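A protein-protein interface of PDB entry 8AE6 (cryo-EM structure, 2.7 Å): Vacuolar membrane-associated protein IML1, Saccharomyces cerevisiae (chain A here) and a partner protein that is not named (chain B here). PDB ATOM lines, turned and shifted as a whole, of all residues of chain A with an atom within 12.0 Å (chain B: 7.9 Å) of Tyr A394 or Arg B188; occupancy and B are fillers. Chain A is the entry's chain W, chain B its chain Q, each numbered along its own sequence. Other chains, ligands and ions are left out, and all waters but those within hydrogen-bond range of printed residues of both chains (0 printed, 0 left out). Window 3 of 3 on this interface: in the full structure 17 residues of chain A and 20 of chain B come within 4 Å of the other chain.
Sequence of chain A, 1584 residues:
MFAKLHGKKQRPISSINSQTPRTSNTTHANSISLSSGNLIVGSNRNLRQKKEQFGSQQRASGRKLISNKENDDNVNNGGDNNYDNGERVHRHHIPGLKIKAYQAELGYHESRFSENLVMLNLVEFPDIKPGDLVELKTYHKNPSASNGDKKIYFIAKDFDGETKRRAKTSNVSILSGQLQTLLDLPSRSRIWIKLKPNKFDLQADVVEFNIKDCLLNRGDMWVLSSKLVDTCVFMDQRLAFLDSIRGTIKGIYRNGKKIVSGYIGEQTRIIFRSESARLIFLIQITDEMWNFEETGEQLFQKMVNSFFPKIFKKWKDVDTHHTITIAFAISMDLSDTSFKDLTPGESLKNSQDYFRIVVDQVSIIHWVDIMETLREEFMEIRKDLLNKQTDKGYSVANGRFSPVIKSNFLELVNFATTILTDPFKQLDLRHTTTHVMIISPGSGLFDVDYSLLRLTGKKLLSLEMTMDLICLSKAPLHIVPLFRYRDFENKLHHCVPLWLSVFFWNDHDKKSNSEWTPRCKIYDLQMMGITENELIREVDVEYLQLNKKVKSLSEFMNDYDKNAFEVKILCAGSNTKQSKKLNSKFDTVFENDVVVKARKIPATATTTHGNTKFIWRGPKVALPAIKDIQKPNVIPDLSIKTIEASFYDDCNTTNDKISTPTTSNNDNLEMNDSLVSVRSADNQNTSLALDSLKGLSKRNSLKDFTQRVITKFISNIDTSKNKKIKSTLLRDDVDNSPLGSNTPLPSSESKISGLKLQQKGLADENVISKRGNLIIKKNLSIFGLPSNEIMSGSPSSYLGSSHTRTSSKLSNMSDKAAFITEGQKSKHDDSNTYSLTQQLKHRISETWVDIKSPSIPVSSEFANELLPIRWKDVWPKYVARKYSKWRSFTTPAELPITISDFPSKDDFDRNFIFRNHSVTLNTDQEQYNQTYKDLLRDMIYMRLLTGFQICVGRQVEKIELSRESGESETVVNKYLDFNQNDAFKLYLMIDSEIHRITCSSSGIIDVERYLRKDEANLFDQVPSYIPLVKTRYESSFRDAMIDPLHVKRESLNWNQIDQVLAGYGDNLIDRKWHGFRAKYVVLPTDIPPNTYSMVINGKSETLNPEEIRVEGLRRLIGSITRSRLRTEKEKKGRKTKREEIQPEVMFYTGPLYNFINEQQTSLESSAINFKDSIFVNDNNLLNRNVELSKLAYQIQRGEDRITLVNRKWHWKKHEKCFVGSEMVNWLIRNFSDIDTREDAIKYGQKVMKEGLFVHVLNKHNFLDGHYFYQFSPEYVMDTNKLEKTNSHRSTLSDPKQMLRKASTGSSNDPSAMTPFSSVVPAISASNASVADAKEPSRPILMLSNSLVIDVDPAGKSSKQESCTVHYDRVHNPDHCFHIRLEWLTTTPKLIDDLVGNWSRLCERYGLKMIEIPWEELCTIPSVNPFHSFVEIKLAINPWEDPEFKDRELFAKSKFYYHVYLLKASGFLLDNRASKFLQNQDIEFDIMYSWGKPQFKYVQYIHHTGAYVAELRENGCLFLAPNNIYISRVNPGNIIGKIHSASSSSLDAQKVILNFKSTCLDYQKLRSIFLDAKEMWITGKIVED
Tyr A394 touches four residues of chain B.
No residue of chain B comes within 4 Å of Gly A393.
No residue of chain A comes within 4 Å of Asp B186.
No residue of chain A comes within 4 Å of Leu B187.
Of chain A, only Tyr A394 (3.2 Å) comes within 4 Å of Lys B189.
Gly B190 touches just these residues of chain A: Tyr A394 and Ser A395.
Ser B191 touches two residues of chain A.
Thr B192 touches two residues of chain A.
Printed residues of chain B within 4 Å of Asn A387: Ser B191.
Printed residues of chain B within 4 Å of Ser A395: Gly B190, Ser B191 and Thr B192.
Asp A391 touches none of the printed residues of chain B.
Pro B193 touches none of the printed residues of chain A.
The nearest residue of chain B that does not touch Tyr A394 is Ser B191 (5.1 Å).
The nearest printed residue of chain B that does not touch Ser A395 is Lys B189 (4.2 Å).
The side-chain carboxylate of Asp B186 is in salt-bridge range of the guanidinium group of Arg B188 (2.9 Å).
The backbone carbonyl oxygen of Lys A388 lies within hydrogen-bond range of the side-chain hydroxyl of Ser A395 (2.4 Å).
The side-chain hydroxyl (OG1) of Thr B192 sits at hydrogen-bond distance from the backbone carbonyl oxygen (O) of Lys B189.
The side-chain amide nitrogen (ND2) of Asn B172 sits close to the guanidinium group (NE) of Arg B188 (3.4 Å).
The side-chain hydroxyl (OG) of Ser A395 lies close to the side-chain amide nitrogen (ND2) of Asn A387.
The side-chain hydroxyl of Tyr B152 lies within hydrogen-bond range of the backbone carbonyl oxygen of Gly B190, at 2.6 Å.
OG of Ser B191 sits at hydrogen-bond distance from O of Ser A395.
The side-chain amide oxygen of Asn A387 sits at hydrogen-bond distance from the side-chain hydroxyl of Ser B191, at 2.7 Å.
Among the printed residues, pairs that only touch across the chains: Tyr A394 with Lys B189 (3.2 Å), Ser A395 with Gly B190 (3.3 Å), Tyr A394 with Thr B192 (3.3 Å), Tyr A394 with Gly B190 (3.6 Å), Ser A395 with Thr B192 (3.6 Å) and Tyr A394 with Arg B188 (3.7 Å).
Of the 16 printed residues of chain B, 5 touch a printed residue of chain A.
Among the printed residues, no Asp or Glu carboxylate lies within 4 Å of a Lys or Arg side-chain nitrogen of the other chain.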
ATOM      1  N   LYS A 383      25.613  -0.343  12.321  1.00  0.00           N
ATOM      2  CA  LYS A 383      26.393  -0.429  13.549  1.00  0.00           C
ATOM      3  C   LYS A 383      27.080   0.891  13.863  1.00  0.00           C
ATOM      4  O   LYS A 383      27.230   1.244  15.038  1.00  0.00           O
ATOM      5  CB  LYS A 383      27.425  -1.548  13.438  1.00  0.00           C
ATOM      6  CG  LYS A 383      28.187  -1.834  14.721  1.00  0.00           C
ATOM      7  CD  LYS A 383      29.300  -2.841  14.499  1.00  0.00           C
ATOM      8  CE  LYS A 383      29.611  -3.603  15.777  1.00  0.00           C
ATOM      9  NZ  LYS A 383      29.384  -2.771  16.991  1.00  0.00           N
ATOM     10  N   LEU A 385      25.990   3.960  13.266  1.00  0.00           N
ATOM     11  CA  LEU A 385      25.104   5.034  13.701  1.00  0.00           C
ATOM     12  C   LEU A 385      24.141   4.636  14.814  1.00  0.00           C
ATOM     13  O   LEU A 385      23.962   5.396  15.768  1.00  0.00           O
ATOM     14  CB  LEU A 385      24.324   5.574  12.501  1.00  0.00           C
ATOM     15  CG  LEU A 385      25.250   6.298  11.537  1.00  0.00           C
ATOM     16  CD1 LEU A 385      24.581   6.466  10.205  1.00  0.00           C
ATOM     17  CD2 LEU A 385      25.639   7.637  12.109  1.00  0.00           C
ATOM     18  N   LEU A 386      23.515   3.468  14.725  1.00  0.00           N
ATOM     19  CA  LEU A 386      22.465   3.117  15.673  1.00  0.00           C
ATOM     20  C   LEU A 386      22.991   2.506  16.963  1.00  0.00           C
ATOM     21  O   LEU A 386      22.184   2.118  17.816  1.00  0.00           O
ATOM     22  CB  LEU A 386      21.468   2.160  15.017  1.00  0.00           C
ATOM     23  CG  LEU A 386      20.726   2.717  13.802  1.00  0.00           C
ATOM     24  CD1 LEU A 386      19.711   1.721  13.289  1.00  0.00           C
ATOM     25  CD2 LEU A 386      20.059   4.039  14.135  1.00  0.00           C
ATOM     26  N   ASN A 387      24.305   2.403  17.134  1.00  0.00           N
ATOM     27  CA  ASN A 387      24.917   1.923  18.370  1.00  0.00           C
ATOM     28  C   ASN A 387      25.672   3.093  18.992  1.00  0.00           C
ATOM     29  O   ASN A 387      26.874   3.260  18.777  1.00  0.00           O
ATOM     30  CB  ASN A 387      25.845   0.746  18.101  1.00  0.00           C
ATOM     31  CG  ASN A 387      25.711  -0.350  19.128  1.00  0.00           C
ATOM     32  OD1 ASN A 387      24.640  -0.548  19.698  1.00  0.00           O
ATOM     33  ND2 ASN A 387      26.796  -1.070  19.370  1.00  0.00           N
ATOM     34  N   LYS A 388      24.960   3.910  19.763  1.00  0.00           N
ATOM     35  CA  LYS A 388      25.598   5.054  20.392  1.00  0.00           C
ATOM     36  C   LYS A 388      26.415   4.604  21.599  1.00  0.00           C
ATOM     37  O   LYS A 388      26.158   3.562  22.203  1.00  0.00           O
ATOM     38  CB  LYS A 388      24.562   6.103  20.803  1.00  0.00           C
ATOM     39  CG  LYS A 388      23.754   5.761  22.044  1.00  0.00           C
ATOM     40  CD  LYS A 388      22.791   6.880  22.402  1.00  0.00           C
ATOM     41  CE  LYS A 388      22.158   6.647  23.764  1.00  0.00           C
ATOM     42  NZ  LYS A 388      21.218   7.740  24.134  1.00  0.00           N
ATOM     43  N   GLN A 389      27.423   5.403  21.935  1.00  0.00           N
ATOM     44  CA  GLN A 389      28.340   5.088  23.021  1.00  0.00           C
ATOM     45  C   GLN A 389      27.969   5.907  24.249  1.00  0.00           C
ATOM     46  O   GLN A 389      27.945   7.143  24.194  1.00  0.00           O
ATOM     47  CB  GLN A 389      29.785   5.364  22.611  1.00  0.00           C
ATOM     48  CG  GLN A 389      30.804   5.040  23.687  1.00  0.00           C
ATOM     49  CD  GLN A 389      30.903   3.555  23.968  1.00  0.00           C
ATOM     50  OE1 GLN A 389      30.803   2.733  23.055  1.00  0.00           O
ATOM     51  NE2 GLN A 389      31.103   3.202  25.231  1.00  0.00           N
ATOM     52  N   THR A 390      27.679   5.221  25.349  1.00  0.00           N
ATOM     53  CA  THR A 390      27.377   5.873  26.614  1.00  0.00           C
ATOM     54  C   THR A 390      28.654   5.974  27.438  1.00  0.00           C
ATOM     55  O   THR A 390      29.529   5.107  27.355  1.00  0.00           O
ATOM     56  CB  THR A 390      26.301   5.093  27.377  1.00  0.00           C
ATOM     57  OG1 THR A 390      25.278   4.680  26.462  1.00  0.00           O
ATOM     58  CG2 THR A 390      25.656   5.954  28.457  1.00  0.00           C
ATOM     59  N   ASP A 391      28.759   7.042  28.234  1.00  0.00           N
ATOM     60  CA  ASP A 391      29.954   7.295  29.031  1.00  0.00           C
ATOM     61  C   ASP A 391      30.120   6.322  30.193  1.00  0.00           C
ATOM     62  O   ASP A 391      31.174   6.336  30.839  1.00  0.00           O
ATOM     63  CB  ASP A 391      29.932   8.730  29.562  1.00  0.00           C
ATOM     64  CG  ASP A 391      29.781   9.756  28.458  1.00  0.00           C
ATOM     65  OD1 ASP A 391      29.736   9.356  27.275  1.00  0.00           O
ATOM     66  OD2 ASP A 391      29.707  10.964  28.772  1.00  0.00           O
ATOM     67  N   LYS A 392      29.121   5.487  30.476  1.00  0.00           N
ATOM     68  CA  LYS A 392      29.189   4.530  31.570  1.00  0.00           C
ATOM     69  C   LYS A 392      30.028   3.299  31.244  1.00  0.00           C
ATOM     70  O   LYS A 392      30.137   2.406  32.090  1.00  0.00           O
ATOM     71  CB  LYS A 392      27.778   4.094  31.970  1.00  0.00           C
ATOM     72  CG  LYS A 392      26.791   5.239  32.107  1.00  0.00           C
ATOM     73  CD  LYS A 392      25.416   4.733  32.518  1.00  0.00           C
ATOM     74  CE  LYS A 392      24.506   5.879  32.921  1.00  0.00           C
ATOM     75  NZ  LYS A 392      23.196   5.392  33.438  1.00  0.00           N
ATOM     76  N   GLY A 393      30.613   3.222  30.051  1.00  0.00           N
ATOM     77  CA  GLY A 393      31.462   2.112  29.678  1.00  0.00           C
ATOM     78  C   GLY A 393      30.827   1.092  28.761  1.00  0.00           C
ATOM     79  O   GLY A 393      31.456   0.068  28.475  1.00  0.00           O
ATOM     80  N   TYR A 394      29.604   1.336  28.291  1.00  0.00           N
ATOM     81  CA  TYR A 394      28.921   0.409  27.404  1.00  0.00           C
ATOM     82  C   TYR A 394      28.142   1.195  26.359  1.00  0.00           C
ATOM     83  O   TYR A 394      27.999   2.416  26.445  1.00  0.00           O
ATOM     84  CB  TYR A 394      28.014  -0.545  28.188  1.00  0.00           C
ATOM     85  CG  TYR A 394      26.932   0.114  29.022  1.00  0.00           C
ATOM     86  CD1 TYR A 394      25.676   0.381  28.489  1.00  0.00           C
ATOM     87  CD2 TYR A 394      27.160   0.440  30.353  1.00  0.00           C
ATOM     88  CE1 TYR A 394      24.688   0.974  29.251  1.00  0.00           C
ATOM     89  CE2 TYR A 394      26.176   1.029  31.121  1.00  0.00           C
ATOM     90  CZ  TYR A 394      24.945   1.296  30.564  1.00  0.00           C
ATOM     91  OH  TYR A 394      23.962   1.884  31.328  1.00  0.00           O
ATOM     92  N   SER A 395      27.631   0.476  25.362  1.00  0.00           N
ATOM     93  CA  SER A 395      26.942   1.071  24.226  1.00  0.00           C
ATOM     94  C   SER A 395      25.468   0.696  24.253  1.00  0.00           C
ATOM     95  O   SER A 395      25.115  -0.450  24.537  1.00  0.00           O
ATOM     96  CB  SER A 395      27.570   0.618  22.906  1.00  0.00           C
ATOM     97  OG  SER A 395      27.043   1.351  21.814  1.00  0.00           O
ATOM     98  N   VAL A 396      24.611   1.667  23.947  1.00  0.00           N
ATOM     99  CA  VAL A 396      23.162   1.502  23.984  1.00  0.00           C
ATOM    100  C   VAL A 396      22.627   1.616  22.564  1.00  0.00           C
ATOM    101  O   VAL A 396      22.949   2.570  21.849  1.00  0.00           O
ATOM    102  CB  VAL A 396      22.506   2.541  24.911  1.00  0.00           C
ATOM    103  CG1 VAL A 396      20.991   2.508  24.783  1.00  0.00           C
ATOM    104  CG2 VAL A 396      22.923   2.302  26.350  1.00  0.00           C
ATOM    105  N   ALA A 397      21.814   0.642  22.155  1.00  0.00           N
ATOM    106  CA  ALA A 397      21.203   0.664  20.831  1.00  0.00           C
ATOM    107  C   ALA A 397      20.110   1.721  20.762  1.00  0.00           C
ATOM    108  O   ALA A 397      18.965   1.467  21.151  1.00  0.00           O
ATOM    109  CB  ALA A 397      20.634  -0.711  20.475  1.00  0.00           C
ATOM    110  N   ASN A 398      20.453   2.907  20.268  1.00  0.00           N
ATOM    111  CA  ASN A 398      19.532   4.031  20.227  1.00  0.00           C
ATOM    112  C   ASN A 398      19.725   4.794  18.925  1.00  0.00           C
ATOM    113  O   ASN A 398      20.762   4.687  18.265  1.00  0.00           O
ATOM    114  CB  ASN A 398      19.734   4.967  21.428  1.00  0.00           C
ATOM    115  CG  ASN A 398      18.488   5.762  21.764  1.00  0.00           C
ATOM    116  OD1 ASN A 398      17.392   5.449  21.298  1.00  0.00           O
ATOM    117  ND2 ASN A 398      18.652   6.798  22.578  1.00  0.00           N
ATOM    118  N   TYR B 152      14.694  -2.864  26.467  1.00  0.00           N
ATOM    119  CA  TYR B 152      16.071  -3.223  26.160  1.00  0.00           C
ATOM    120  C   TYR B 152      16.158  -3.561  24.684  1.00  0.00           C
ATOM    121  O   TYR B 152      15.347  -4.343  24.176  1.00  0.00           O
ATOM    122  CB  TYR B 152      16.531  -4.412  27.005  1.00  0.00           C
ATOM    123  CG  TYR B 152      17.918  -4.909  26.681  1.00  0.00           C
ATOM    124  CD1 TYR B 152      19.039  -4.190  27.064  1.00  0.00           C
ATOM    125  CD2 TYR B 152      18.109  -6.100  25.993  1.00  0.00           C
ATOM    126  CE1 TYR B 152      20.307  -4.642  26.776  1.00  0.00           C
ATOM    127  CE2 TYR B 152      19.375  -6.559  25.701  1.00  0.00           C
ATOM    128  CZ  TYR B 152      20.468  -5.824  26.094  1.00  0.00           C
ATOM    129  OH  TYR B 152      21.736  -6.268  25.806  1.00  0.00           O
ATOM    130  N   ASP B 170      20.983 -16.177  36.613  1.00  0.00           N
ATOM    131  CA  ASP B 170      21.216 -14.745  36.668  1.00  0.00           C
ATOM    132  C   ASP B 170      20.122 -14.056  35.856  1.00  0.00           C
ATOM    133  O   ASP B 170      20.102 -14.192  34.627  1.00  0.00           O
ATOM    134  CB  ASP B 170      22.604 -14.450  36.113  1.00  0.00           C
ATOM    135  CG  ASP B 170      23.047 -13.022  36.330  1.00  0.00           C
ATOM    136  OD1 ASP B 170      22.283 -12.218  36.888  1.00  0.00           O
ATOM    137  OD2 ASP B 170      24.190 -12.700  35.956  1.00  0.00           O
ATOM    138  N   PRO B 171      19.205 -13.316  36.483  1.00  0.00           N
ATOM    139  CA  PRO B 171      17.965 -12.913  35.803  1.00  0.00           C
ATOM    140  C   PRO B 171      18.076 -11.693  34.902  1.00  0.00           C
ATOM    141  O   PRO B 171      17.040 -11.125  34.547  1.00  0.00           O
ATOM    142  CB  PRO B 171      16.998 -12.635  36.970  1.00  0.00           C
ATOM    143  CG  PRO B 171      17.826 -12.653  38.230  1.00  0.00           C
ATOM    144  CD  PRO B 171      19.264 -12.795  37.858  1.00  0.00           C
ATOM    145  N   ASN B 172      19.275 -11.272  34.514  1.00  0.00           N
ATOM    146  CA  ASN B 172      19.414 -10.205  33.532  1.00  0.00           C
ATOM    147  C   ASN B 172      20.543 -10.507  32.552  1.00  0.00           C
ATOM    148  O   ASN B 172      21.228  -9.593  32.081  1.00  0.00           O
ATOM    149  CB  ASN B 172      19.608  -8.852  34.217  1.00  0.00           C
ATOM    150  CG  ASN B 172      20.592  -8.909  35.348  1.00  0.00           C
ATOM    151  OD1 ASN B 172      21.262  -9.917  35.547  1.00  0.00           O
ATOM    152  ND2 ASN B 172      20.667  -7.835  36.114  1.00  0.00           N
ATOM    153  N   VAL B 173      20.745 -11.783  32.237  1.00  0.00           N
ATOM    154  CA  VAL B 173      21.708 -12.225  31.237  1.00  0.00           C
ATOM    155  C   VAL B 173      20.961 -13.055  30.202  1.00  0.00           C
ATOM    156  O   VAL B 173      20.294 -14.033  30.554  1.00  0.00           O
ATOM    157  CB  VAL B 173      22.851 -13.040  31.872  1.00  0.00           C
ATOM    158  CG1 VAL B 173      23.618 -13.811  30.814  1.00  0.00           C
ATOM    159  CG2 VAL B 173      23.782 -12.121  32.634  1.00  0.00           C
ATOM    160  N   LEU B 174      21.058 -12.658  28.936  1.00  0.00           N
ATOM    161  CA  LEU B 174      20.408 -13.387  27.858  1.00  0.00           C
ATOM    162  C   LEU B 174      21.373 -13.520  26.691  1.00  0.00           C
ATOM    163  O   LEU B 174      22.202 -12.640  26.449  1.00  0.00           O
ATOM    164  CB  LEU B 174      19.102 -12.711  27.399  1.00  0.00           C
ATOM    165  CG  LEU B 174      19.087 -11.416  26.588  1.00  0.00           C
ATOM    166  CD1 LEU B 174      17.722 -11.239  25.976  1.00  0.00           C
ATOM    167  CD2 LEU B 174      19.429 -10.195  27.419  1.00  0.00           C
ATOM    168  N   TRP B 185      24.417 -11.348  26.198  1.00  0.00           N
ATOM    169  CA  TRP B 185      24.110  -9.974  26.563  1.00  0.00           C
ATOM    170  C   TRP B 185      23.826  -9.866  28.052  1.00  0.00           C
ATOM    171  O   TRP B 185      23.169 -10.730  28.637  1.00  0.00           O
ATOM    172  CB  TRP B 185      22.896  -9.446  25.794  1.00  0.00           C
ATOM    173  CG  TRP B 185      22.799  -9.875  24.368  1.00  0.00           C
ATOM    174  CD1 TRP B 185      22.006 -10.857  23.861  1.00  0.00           C
ATOM    175  CD2 TRP B 185      23.501  -9.313  23.256  1.00  0.00           C
ATOM    176  NE1 TRP B 185      22.177 -10.950  22.505  1.00  0.00           N
ATOM    177  CE2 TRP B 185      23.090 -10.011  22.108  1.00  0.00           C
ATOM    178  CE3 TRP B 185      24.440  -8.290  23.123  1.00  0.00           C
ATOM    179  CZ2 TRP B 185      23.586  -9.720  20.846  1.00  0.00           C
ATOM    180  CZ3 TRP B 185      24.932  -8.006  21.871  1.00  0.00           C
ATOM    181  CH2 TRP B 185      24.505  -8.715  20.749  1.00  0.00           C
ATOM    182  N   ASP B 186      24.329  -8.800  28.660  1.00  0.00           N
ATOM    183  CA  ASP B 186      23.934  -8.398  29.999  1.00  0.00           C
ATOM    184  C   ASP B 186      22.917  -7.274  29.871  1.00  0.00           C
ATOM    185  O   ASP B 186      23.137  -6.314  29.123  1.00  0.00           O
ATOM    186  CB  ASP B 186      25.141  -7.940  30.819  1.00  0.00           C
ATOM    187  CG  ASP B 186      24.887  -7.984  32.312  1.00  0.00           C
ATOM    188  OD1 ASP B 186      23.769  -8.359  32.718  1.00  0.00           O
ATOM    189  OD2 ASP B 186      25.809  -7.642  33.081  1.00  0.00           O
ATOM    190  N   LEU B 187      21.803  -7.399  30.593  1.00  0.00           N
ATOM    191  CA  LEU B 187      20.697  -6.463  30.433  1.00  0.00           C
ATOM    192  C   LEU B 187      21.018  -5.082  30.997  1.00  0.00           C
ATOM    193  O   LEU B 187      20.341  -4.115  30.637  1.00  0.00           O
ATOM    194  CB  LEU B 187      19.452  -7.039  31.101  1.00  0.00           C
ATOM    195  CG  LEU B 187      18.042  -6.596  30.740  1.00  0.00           C
ATOM    196  CD1 LEU B 187      17.676  -7.138  29.384  1.00  0.00           C
ATOM    197  CD2 LEU B 187      17.066  -7.097  31.787  1.00  0.00           C
ATOM    198  N   ARG B 188      22.023  -4.970  31.865  1.00  0.00           N
ATOM    199  CA  ARG B 188      22.481  -3.680  32.369  1.00  0.00           C
ATOM    200  C   ARG B 188      23.708  -3.153  31.639  1.00  0.00           C
ATOM    201  O   ARG B 188      24.210  -2.086  32.002  1.00  0.00           O
ATOM    202  CB  ARG B 188      22.801  -3.757  33.863  1.00  0.00           C
ATOM    203  CG  ARG B 188      21.804  -4.506  34.708  1.00  0.00           C
ATOM    204  CD  ARG B 188      22.514  -5.103  35.909  1.00  0.00           C
ATOM    205  NE  ARG B 188      23.521  -6.077  35.511  1.00  0.00           N
ATOM    206  CZ  ARG B 188      24.274  -6.765  36.357  1.00  0.00           C
ATOM    207  NH1 ARG B 188      24.176  -6.594  37.665  1.00  0.00           N
ATOM    208  NH2 ARG B 188      25.150  -7.643  35.880  1.00  0.00           N
ATOM    209  N   LYS B 189      24.207  -3.866  30.631  1.00  0.00           N
ATOM    210  CA  LYS B 189      25.414  -3.460  29.927  1.00  0.00           C
ATOM    211  C   LYS B 189      25.140  -3.033  28.491  1.00  0.00           C
ATOM    212  O   LYS B 189      26.055  -3.035  27.663  1.00  0.00           O
ATOM    213  CB  LYS B 189      26.450  -4.585  29.957  1.00  0.00           C
ATOM    214  CG  LYS B 189      27.113  -4.756  31.311  1.00  0.00           C
ATOM    215  CD  LYS B 189      28.346  -5.634  31.227  1.00  0.00           C
ATOM    216  CE  LYS B 189      29.035  -5.724  32.580  1.00  0.00           C
ATOM    217  NZ  LYS B 189      30.269  -6.554  32.533  1.00  0.00           N
ATOM    218  N   GLY B 190      23.894  -2.675  28.178  1.00  0.00           N
ATOM    219  CA  GLY B 190      23.577  -2.134  26.865  1.00  0.00           C
ATOM    220  C   GLY B 190      23.736  -3.151  25.752  1.00  0.00           C
ATOM    221  O   GLY B 190      23.409  -4.335  25.899  1.00  0.00           O
ATOM    222  N   SER B 191      24.251  -2.685  24.617  1.00  0.00           N
ATOM    223  CA  SER B 191      24.456  -3.532  23.452  1.00  0.00           C
ATOM    224  C   SER B 191      25.820  -4.210  23.429  1.00  0.00           C
ATOM    225  O   SER B 191      26.054  -5.054  22.557  1.00  0.00           O
ATOM    226  CB  SER B 191      24.280  -2.714  22.170  1.00  0.00           C
ATOM    227  OG  SER B 191      25.424  -1.920  21.914  1.00  0.00           O
ATOM    228  N   THR B 192      26.718  -3.870  24.342  1.00  0.00           N
ATOM    229  CA  THR B 192      28.019  -4.525  24.376  1.00  0.00           C
ATOM    230  C   THR B 192      27.880  -5.912  24.987  1.00  0.00           C
ATOM    231  O   THR B 192      27.379  -6.041  26.107  1.00  0.00           O
ATOM    232  CB  THR B 192      29.024  -3.706  25.175  1.00  0.00           C
ATOM    233  OG1 THR B 192      28.444  -3.331  26.430  1.00  0.00           O
ATOM    234  CG2 THR B 192      29.416  -2.451  24.411  1.00  0.00           C
ATOM    235  N   PRO B 193      28.299  -6.962  24.292  1.00  0.00           N
ATOM    236  CA  PRO B 193      28.123  -8.316  24.818  1.00  0.00           C
ATOM    237  C   PRO B 193      29.092  -8.629  25.946  1.00  0.00           C
ATOM    238  O   PRO B 193      30.212  -8.116  26.004  1.00  0.00           O
ATOM    239  CB  PRO B 193      28.398  -9.212  23.601  1.00  0.00           C
ATOM    240  CG  PRO B 193      28.559  -8.292  22.431  1.00  0.00           C
ATOM    241  CD  PRO B 193      28.948  -6.968  22.974  1.00  0.00           C
ATOM    242  N   LEU B 194      28.625  -9.475  26.865  1.00  0.00           N
ATOM    243  CA  LEU B 194      29.499 -10.000  27.904  1.00  0.00           C
ATOM    244  C   LEU B 194      30.586 -10.882  27.308  1.00  0.00           C
ATOM    245  O   LEU B 194      31.752 -10.806  27.716  1.00  0.00           O
ATOM    246  CB  LEU B 194      28.683 -10.784  28.930  1.00  0.00           C
ATOM    247  CG  LEU B 194      28.241 -10.043  30.187  1.00  0.00           C
ATOM    248  CD1 LEU B 194      27.391 -10.954  31.054  1.00  0.00           C
ATOM    249  CD2 LEU B 194      29.444  -9.532  30.961  1.00  0.00           C
